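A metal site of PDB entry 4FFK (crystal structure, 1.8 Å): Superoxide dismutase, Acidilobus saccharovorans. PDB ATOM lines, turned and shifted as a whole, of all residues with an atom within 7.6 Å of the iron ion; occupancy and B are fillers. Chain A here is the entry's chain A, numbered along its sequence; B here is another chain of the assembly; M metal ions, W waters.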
ATOM      1  N   HIS A  43      34.163  16.752 -19.869  1.00  0.00           N
ATOM      2  CA  HIS A  43      33.401  15.692 -20.459  1.00  0.00           C
ATOM      3  C   HIS A  43      33.912  15.367 -21.847  1.00  0.00           C
ATOM      4  O   HIS A  43      34.149  14.203 -22.160  1.00  0.00           O
ATOM      5  CB  HIS A  43      31.944  16.088 -20.510  1.00  0.00           C
ATOM      6  CG  HIS A  43      31.045  14.904 -20.673  1.00  0.00           C
ATOM      7  ND1 HIS A  43      29.664  15.006 -20.594  1.00  0.00           N
ATOM      8  CD2 HIS A  43      31.314  13.605 -20.938  1.00  0.00           C
ATOM      9  CE1 HIS A  43      29.131  13.809 -20.776  1.00  0.00           C
ATOM     10  NE2 HIS A  43      30.115  12.937 -20.957  1.00  0.00           N
ATOM     11  N   HIS A  44      34.197  16.412 -22.647  1.00  0.00           N
ATOM     12  CA  HIS A  44      34.617  16.146 -23.960  1.00  0.00           C
ATOM     13  C   HIS A  44      36.091  15.850 -24.050  1.00  0.00           C
ATOM     14  O   HIS A  44      36.478  14.897 -24.692  1.00  0.00           O
ATOM     15  CB  HIS A  44      34.232  17.286 -24.933  1.00  0.00           C
ATOM     16  CG  HIS A  44      34.727  17.056 -26.310  1.00  0.00           C
ATOM     17  ND1 HIS A  44      36.051  17.246 -26.670  1.00  0.00           N
ATOM     18  CD2 HIS A  44      34.087  16.646 -27.417  1.00  0.00           C
ATOM     19  CE1 HIS A  44      36.196  16.939 -27.942  1.00  0.00           C
ATOM     20  NE2 HIS A  44      35.019  16.562 -28.414  1.00  0.00           N
ATOM     21  N   HIS A  47      36.930  12.944 -20.552  1.00  0.00           N
ATOM     22  CA  HIS A  47      36.227  11.623 -20.512  1.00  0.00           C
ATOM     23  C   HIS A  47      36.090  11.073 -21.890  1.00  0.00           C
ATOM     24  O   HIS A  47      36.495   9.959 -22.119  1.00  0.00           O
ATOM     25  CB  HIS A  47      34.816  11.770 -19.896  1.00  0.00           C
ATOM     26  CG  HIS A  47      34.859  12.080 -18.463  1.00  0.00           C
ATOM     27  ND1 HIS A  47      35.225  11.142 -17.519  1.00  0.00           N
ATOM     28  CD2 HIS A  47      34.638  13.226 -17.797  1.00  0.00           C
ATOM     29  CE1 HIS A  47      35.214  11.709 -16.325  1.00  0.00           C
ATOM     30  NE2 HIS A  47      34.859  12.968 -16.461  1.00  0.00           N
ATOM     31  N   HIS A  48      35.569  11.841 -22.872  1.00  0.00           N
ATOM     32  CA  HIS A  48      35.362  11.300 -24.193  1.00  0.00           C
ATOM     33  C   HIS A  48      36.731  10.876 -24.772  1.00  0.00           C
ATOM     34  O   HIS A  48      36.864   9.792 -25.299  1.00  0.00           O
ATOM     35  CB  HIS A  48      34.638  12.289 -25.107  1.00  0.00           C
ATOM     36  CG  HIS A  48      34.334  11.768 -26.470  1.00  0.00           C
ATOM     37  ND1 HIS A  48      33.515  12.443 -27.328  1.00  0.00           N
ATOM     38  CD2 HIS A  48      34.654  10.610 -27.091  1.00  0.00           C
ATOM     39  CE1 HIS A  48      33.401  11.765 -28.452  1.00  0.00           C
ATOM     40  NE2 HIS A  48      34.041  10.616 -28.306  1.00  0.00           N
ATOM     41  N   TYR A  51      37.805   7.479 -23.506  1.00  0.00           N
ATOM     42  CA  TYR A  51      37.195   6.353 -24.268  1.00  0.00           C
ATOM     43  C   TYR A  51      37.804   6.133 -25.649  1.00  0.00           C
ATOM     44  O   TYR A  51      38.125   5.031 -26.052  1.00  0.00           O
ATOM     45  CB  TYR A  51      35.663   6.501 -24.363  1.00  0.00           C
ATOM     46  CG  TYR A  51      35.069   6.702 -23.001  1.00  0.00           C
ATOM     47  CD1 TYR A  51      35.356   5.816 -21.923  1.00  0.00           C
ATOM     48  CD2 TYR A  51      34.240   7.838 -22.741  1.00  0.00           C
ATOM     49  CE1 TYR A  51      34.825   6.069 -20.639  1.00  0.00           C
ATOM     50  CE2 TYR A  51      33.709   8.058 -21.488  1.00  0.00           C
ATOM     51  CZ  TYR A  51      33.975   7.169 -20.461  1.00  0.00           C
ATOM     52  OH  TYR A  51      33.386   7.413 -19.256  1.00  0.00           O
ATOM     53  N   GLY A  88      31.748   4.105 -25.477  1.00  0.00           N
ATOM     54  CA  GLY A  88      31.977   5.431 -24.901  1.00  0.00           C
ATOM     55  C   GLY A  88      32.195   6.437 -26.009  1.00  0.00           C
ATOM     56  O   GLY A  88      31.538   7.458 -26.098  1.00  0.00           O
ATOM     57  N   LEU A  91      28.902   6.823 -28.327  1.00  0.00           N
ATOM     58  CA  LEU A  91      27.777   7.419 -27.628  1.00  0.00           C
ATOM     59  C   LEU A  91      28.072   8.869 -27.277  1.00  0.00           C
ATOM     60  O   LEU A  91      27.155   9.712 -27.306  1.00  0.00           O
ATOM     61  CB  LEU A  91      27.420   6.613 -26.382  1.00  0.00           C
ATOM     62  CG  LEU A  91      26.820   5.270 -26.789  1.00  0.00           C
ATOM     63  CD1 LEU A  91      26.646   4.479 -25.461  1.00  0.00           C
ATOM     64  CD2 LEU A  91      25.481   5.493 -27.516  1.00  0.00           C
ATOM     65  N   HIS A  92      29.315   9.201 -26.956  1.00  0.00           N
ATOM     66  CA  HIS A  92      29.612  10.616 -26.669  1.00  0.00           C
ATOM     67  C   HIS A  92      29.499  11.393 -27.935  1.00  0.00           C
ATOM     68  O   HIS A  92      28.946  12.504 -27.927  1.00  0.00           O
ATOM     69  CB  HIS A  92      30.961  10.821 -26.044  1.00  0.00           C
ATOM     70  CG  HIS A  92      30.945  10.484 -24.601  1.00  0.00           C
ATOM     71  ND1 HIS A  92      31.102   9.196 -24.146  1.00  0.00           N
ATOM     72  CD2 HIS A  92      30.725  11.261 -23.521  1.00  0.00           C
ATOM     73  CE1 HIS A  92      30.965   9.191 -22.824  1.00  0.00           C
ATOM     74  NE2 HIS A  92      30.747  10.431 -22.416  1.00  0.00           N
ATOM     75  N   TYR A  95      25.943  11.972 -28.415  1.00  0.00           N
ATOM     76  CA  TYR A  95      25.539  12.930 -27.399  1.00  0.00           C
ATOM     77  C   TYR A  95      25.850  14.384 -27.791  1.00  0.00           C
ATOM     78  O   TYR A  95      24.967  15.219 -27.700  1.00  0.00           O
ATOM     79  CB  TYR A  95      26.288  12.592 -26.149  1.00  0.00           C
ATOM     80  CG  TYR A  95      26.026  13.431 -24.959  1.00  0.00           C
ATOM     81  CD1 TYR A  95      27.069  14.098 -24.333  1.00  0.00           C
ATOM     82  CD2 TYR A  95      24.749  13.451 -24.361  1.00  0.00           C
ATOM     83  CE1 TYR A  95      26.870  14.817 -23.211  1.00  0.00           C
ATOM     84  CE2 TYR A  95      24.553  14.137 -23.196  1.00  0.00           C
ATOM     85  CZ  TYR A  95      25.606  14.858 -22.661  1.00  0.00           C
ATOM     86  OH  TYR A  95      25.424  15.553 -21.539  1.00  0.00           O
ATOM     87  N   TRP A  96      27.081  14.683 -28.177  1.00  0.00           N
ATOM     88  CA  TRP A  96      27.412  16.094 -28.542  1.00  0.00           C
ATOM     89  C   TRP A  96      26.607  16.568 -29.709  1.00  0.00           C
ATOM     90  O   TRP A  96      26.200  17.743 -29.736  1.00  0.00           O
ATOM     91  CB  TRP A  96      28.868  16.254 -28.890  1.00  0.00           C
ATOM     92  CG  TRP A  96      29.804  15.625 -27.941  1.00  0.00           C
ATOM     93  CD1 TRP A  96      30.778  14.717 -28.248  1.00  0.00           C
ATOM     94  CD2 TRP A  96      29.902  15.884 -26.552  1.00  0.00           C
ATOM     95  NE1 TRP A  96      31.495  14.425 -27.138  1.00  0.00           N
ATOM     96  CE2 TRP A  96      30.977  15.083 -26.069  1.00  0.00           C
ATOM     97  CE3 TRP A  96      29.183  16.673 -25.655  1.00  0.00           C
ATOM     98  CZ2 TRP A  96      31.346  15.071 -24.734  1.00  0.00           C
ATOM     99  CZ3 TRP A  96      29.573  16.667 -24.321  1.00  0.00           C
ATOM    100  CH2 TRP A  96      30.639  15.859 -23.881  1.00  0.00           C
ATOM    101  N   GLY A 142      25.188   5.346 -17.257  1.00  0.00           N
ATOM    102  CA  GLY A 142      24.882   4.849 -18.591  1.00  0.00           C
ATOM    103  C   GLY A 142      24.201   5.939 -19.364  1.00  0.00           C
ATOM    104  O   GLY A 142      24.552   7.093 -19.241  1.00  0.00           O
ATOM    105  N   TRP A 143      23.191   5.533 -20.115  1.00  0.00           N
ATOM    106  CA  TRP A 143      22.607   6.395 -21.164  1.00  0.00           C
ATOM    107  C   TRP A 143      21.152   6.015 -21.276  1.00  0.00           C
ATOM    108  O   TRP A 143      20.747   4.880 -21.014  1.00  0.00           O
ATOM    109  CB  TRP A 143      23.178   6.019 -22.524  1.00  0.00           C
ATOM    110  CG  TRP A 143      24.652   6.211 -22.547  1.00  0.00           C
ATOM    111  CD1 TRP A 143      25.580   5.373 -22.053  1.00  0.00           C
ATOM    112  CD2 TRP A 143      25.325   7.365 -23.025  1.00  0.00           C
ATOM    113  NE1 TRP A 143      26.837   5.900 -22.213  1.00  0.00           N
ATOM    114  CE2 TRP A 143      26.708   7.126 -22.840  1.00  0.00           C
ATOM    115  CE3 TRP A 143      24.891   8.571 -23.673  1.00  0.00           C
ATOM    116  CZ2 TRP A 143      27.676   8.035 -23.218  1.00  0.00           C
ATOM    117  CZ3 TRP A 143      25.892   9.483 -24.045  1.00  0.00           C
ATOM    118  CH2 TRP A 143      27.248   9.217 -23.821  1.00  0.00           C
ATOM    119  N   HIS A 163      28.786   1.926 -21.158  1.00  0.00           N
ATOM    120  CA  HIS A 163      28.500   2.232 -22.543  1.00  0.00           C
ATOM    121  C   HIS A 163      28.149   0.994 -23.274  1.00  0.00           C
ATOM    122  O   HIS A 163      27.985   1.037 -24.484  1.00  0.00           O
ATOM    123  CB  HIS A 163      29.770   2.758 -23.203  1.00  0.00           C
ATOM    124  CG  HIS A 163      30.397   3.897 -22.461  1.00  0.00           C
ATOM    125  ND1 HIS A 163      29.669   4.999 -22.037  1.00  0.00           N
ATOM    126  CD2 HIS A 163      31.674   4.099 -22.037  1.00  0.00           C
ATOM    127  CE1 HIS A 163      30.478   5.840 -21.416  1.00  0.00           C
ATOM    128  NE2 HIS A 163      31.697   5.305 -21.381  1.00  0.00           N
ATOM    129  N   ASP A 178      23.577  11.158 -21.871  1.00  0.00           N
ATOM    130  CA  ASP A 178      24.512  10.578 -20.906  1.00  0.00           C
ATOM    131  C   ASP A 178      24.079  10.855 -19.514  1.00  0.00           C
ATOM    132  O   ASP A 178      23.840  12.026 -19.113  1.00  0.00           O
ATOM    133  CB  ASP A 178      25.827  11.291 -21.166  1.00  0.00           C
ATOM    134  CG  ASP A 178      26.984  10.688 -20.465  1.00  0.00           C
ATOM    135  OD1 ASP A 178      26.879   9.670 -19.812  1.00  0.00           O
ATOM    136  OD2 ASP A 178      28.057  11.249 -20.693  1.00  0.00           O
ATOM    137  N   VAL A 179      23.967   9.797 -18.713  1.00  0.00           N
ATOM    138  CA  VAL A 179      23.762   9.954 -17.277  1.00  0.00           C
ATOM    139  C   VAL A 179      24.841   9.302 -16.420  1.00  0.00           C
ATOM    140  O   VAL A 179      24.633   9.003 -15.242  1.00  0.00           O
ATOM    141  CB  VAL A 179      22.387   9.498 -16.832  1.00  0.00           C
ATOM    142  CG1 VAL A 179      21.328  10.349 -17.471  1.00  0.00           C
ATOM    143  CG2 VAL A 179      22.127   7.981 -17.273  1.00  0.00           C
ATOM    144  N   PHE A 180      26.035   9.151 -16.982  1.00  0.00           N
ATOM    145  CA  PHE A 180      27.133   9.062 -16.113  1.00  0.00           C
ATOM    146  C   PHE A 180      27.219  10.339 -15.296  1.00  0.00           C
ATOM    147  O   PHE A 180      26.962  11.415 -15.790  1.00  0.00           O
ATOM    148  CB  PHE A 180      28.413   9.017 -16.888  1.00  0.00           C
ATOM    149  CG  PHE A 180      28.784   7.677 -17.383  1.00  0.00           C
ATOM    150  CD1 PHE A 180      29.985   7.118 -16.908  1.00  0.00           C
ATOM    151  CD2 PHE A 180      27.986   6.998 -18.326  1.00  0.00           C
ATOM    152  CE1 PHE A 180      30.443   5.830 -17.422  1.00  0.00           C
ATOM    153  CE2 PHE A 180      28.402   5.714 -18.790  1.00  0.00           C
ATOM    154  CZ  PHE A 180      29.638   5.180 -18.313  1.00  0.00           C
ATOM    155  N   GLU A 181      27.641  10.196 -14.062  1.00  0.00           N
ATOM    156  CA  GLU A 181      27.651  11.367 -13.192  1.00  0.00           C
ATOM    157  C   GLU A 181      28.478  12.493 -13.756  1.00  0.00           C
ATOM    158  O   GLU A 181      28.205  13.667 -13.529  1.00  0.00           O
ATOM    159  CB  GLU A 181      28.178  10.957 -11.867  1.00  0.00           C
ATOM    160  CG  GLU A 181      27.091  10.148 -11.122  1.00  0.00           C
ATOM    161  CD  GLU A 181      27.598   9.421  -9.934  1.00  0.00           C
ATOM    162  OE1 GLU A 181      28.806   9.141  -9.818  1.00  0.00           O
ATOM    163  OE2 GLU A 181      26.774   9.115  -9.053  1.00  0.00           O
ATOM    164  N   HIS A 182      29.540  12.150 -14.484  1.00  0.00           N
ATOM    165  CA  HIS A 182      30.376  13.246 -14.985  1.00  0.00           C
ATOM    166  C   HIS A 182      29.672  14.154 -16.001  1.00  0.00           C
ATOM    167  O   HIS A 182      30.114  15.291 -16.183  1.00  0.00           O
ATOM    168  CB  HIS A 182      31.678  12.746 -15.587  1.00  0.00           C
ATOM    169  CG  HIS A 182      31.466  11.930 -16.791  1.00  0.00           C
ATOM    170  ND1 HIS A 182      31.798  10.595 -16.823  1.00  0.00           N
ATOM    171  CD2 HIS A 182      30.908  12.226 -17.988  1.00  0.00           C
ATOM    172  CE1 HIS A 182      31.492  10.109 -18.006  1.00  0.00           C
ATOM    173  NE2 HIS A 182      30.977  11.082 -18.746  1.00  0.00           N
ATOM    174  N   ALA A 183      28.557  13.697 -16.571  1.00  0.00           N
ATOM    175  CA  ALA A 183      27.824  14.484 -17.546  1.00  0.00           C
ATOM    176  C   ALA A 183      27.190  15.659 -16.807  1.00  0.00           C
ATOM    177  O   ALA A 183      26.910  16.681 -17.430  1.00  0.00           O
ATOM    178  CB  ALA A 183      26.769  13.645 -18.265  1.00  0.00           C
ATOM    179  N   TYR A 184      26.977  15.517 -15.505  1.00  0.00           N
ATOM    180  CA  TYR A 184      26.128  16.521 -14.796  1.00  0.00           C
ATOM    181  C   TYR A 184      26.635  16.942 -13.484  1.00  0.00           C
ATOM    182  O   TYR A 184      26.138  17.911 -12.894  1.00  0.00           O
ATOM    183  CB  TYR A 184      24.701  16.032 -14.692  1.00  0.00           C
ATOM    184  CG  TYR A 184      24.508  14.717 -14.011  1.00  0.00           C
ATOM    185  CD1 TYR A 184      24.489  14.629 -12.659  1.00  0.00           C
ATOM    186  CD2 TYR A 184      24.297  13.540 -14.755  1.00  0.00           C
ATOM    187  CE1 TYR A 184      24.257  13.421 -11.991  1.00  0.00           C
ATOM    188  CE2 TYR A 184      24.125  12.321 -14.090  1.00  0.00           C
ATOM    189  CZ  TYR A 184      24.071  12.282 -12.739  1.00  0.00           C
ATOM    190  OH  TYR A 184      23.846  11.148 -12.039  1.00  0.00           O
ATOM    191  N   TYR A 195      19.186  17.700 -14.252  1.00  0.00           N
ATOM    192  CA  TYR A 195      19.927  17.664 -15.512  1.00  0.00           C
ATOM    193  C   TYR A 195      19.166  17.127 -16.724  1.00  0.00           C
ATOM    194  O   TYR A 195      19.134  17.772 -17.800  1.00  0.00           O
ATOM    195  CB  TYR A 195      21.225  16.886 -15.269  1.00  0.00           C
ATOM    196  CG  TYR A 195      21.847  16.300 -16.480  1.00  0.00           C
ATOM    197  CD1 TYR A 195      22.547  17.096 -17.401  1.00  0.00           C
ATOM    198  CD2 TYR A 195      21.786  14.924 -16.696  1.00  0.00           C
ATOM    199  CE1 TYR A 195      23.165  16.528 -18.489  1.00  0.00           C
ATOM    200  CE2 TYR A 195      22.358  14.364 -17.817  1.00  0.00           C
ATOM    201  CZ  TYR A 195      23.042  15.130 -18.692  1.00  0.00           C
ATOM    202  OH  TYR A 195      23.627  14.523 -19.766  1.00  0.00           O
ATOM    203  N   GLU B 181      32.053   8.145  -9.821  1.00  0.00           N
ATOM    204  CA  GLU B 181      32.542   9.510  -9.982  1.00  0.00           C
ATOM    205  C   GLU B 181      32.112  10.410  -8.853  1.00  0.00           C
ATOM    206  O   GLU B 181      32.802  11.356  -8.487  1.00  0.00           O
ATOM    207  CB  GLU B 181      32.037  10.034 -11.276  1.00  0.00           C
ATOM    208  CG  GLU B 181      32.837   9.385 -12.428  1.00  0.00           C
ATOM    209  CD  GLU B 181      32.227   9.582 -13.764  1.00  0.00           C
ATOM    210  OE1 GLU B 181      31.014   9.844 -13.885  1.00  0.00           O
ATOM    211  OE2 GLU B 181      32.973   9.491 -14.756  1.00  0.00           O
HETATM  212 FE    FE M   1      29.941  10.867 -20.577  1.00  0.00          FE
HETATM  213  O   HOH W   1      29.542   8.888 -20.207  1.00  0.00           O
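OD2 of Asp 178 binds the iron ion (1.9 Å). The iron ion is bound by water W1, at 2.1 Å. A ring nitrogen (NE2) of His 92 is bound to the iron ion (2.1 Å). NE2 of His 43 is bound to the iron ion, 2.1 Å away. NE2 of His 182 binds the iron ion, 2.1 Å away. The iron ion has five donor atoms within binding distance.
The backbone NH (N) of Phe 180 lies within hydrogen-bond range of the side-chain carboxylate (OD1) of Asp 178, 3.0 Å away. O of Asp 178 lies within hydrogen-bond range of OH of Tyr 195 (2.6 Å). NE1 of Trp 96 lies close to O of His 92 (3.3 Å). A ring nitrogen (ND1) of His 92 sits at hydrogen-bond distance from the backbone carbonyl oxygen (O) of Gly 88 (2.6 Å). The backbone carbonyl oxygen (O) of His 43 lies within hydrogen-bond range of the backbone NH (N) of His 48 (2.8 Å). ND1 of His 182 lies within hydrogen-bond range of OE2 of Glu 181 of chain B, 2.6 Å away.
Within 4 Å of the iron ion: His 43, His 92, Asp 178 and His 182. Along chain A the residues within 4 Å of the iron ion span positions 43 to 182. The nearest printed residue that does not touch the iron ion is Phe 180 (4.4 Å).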
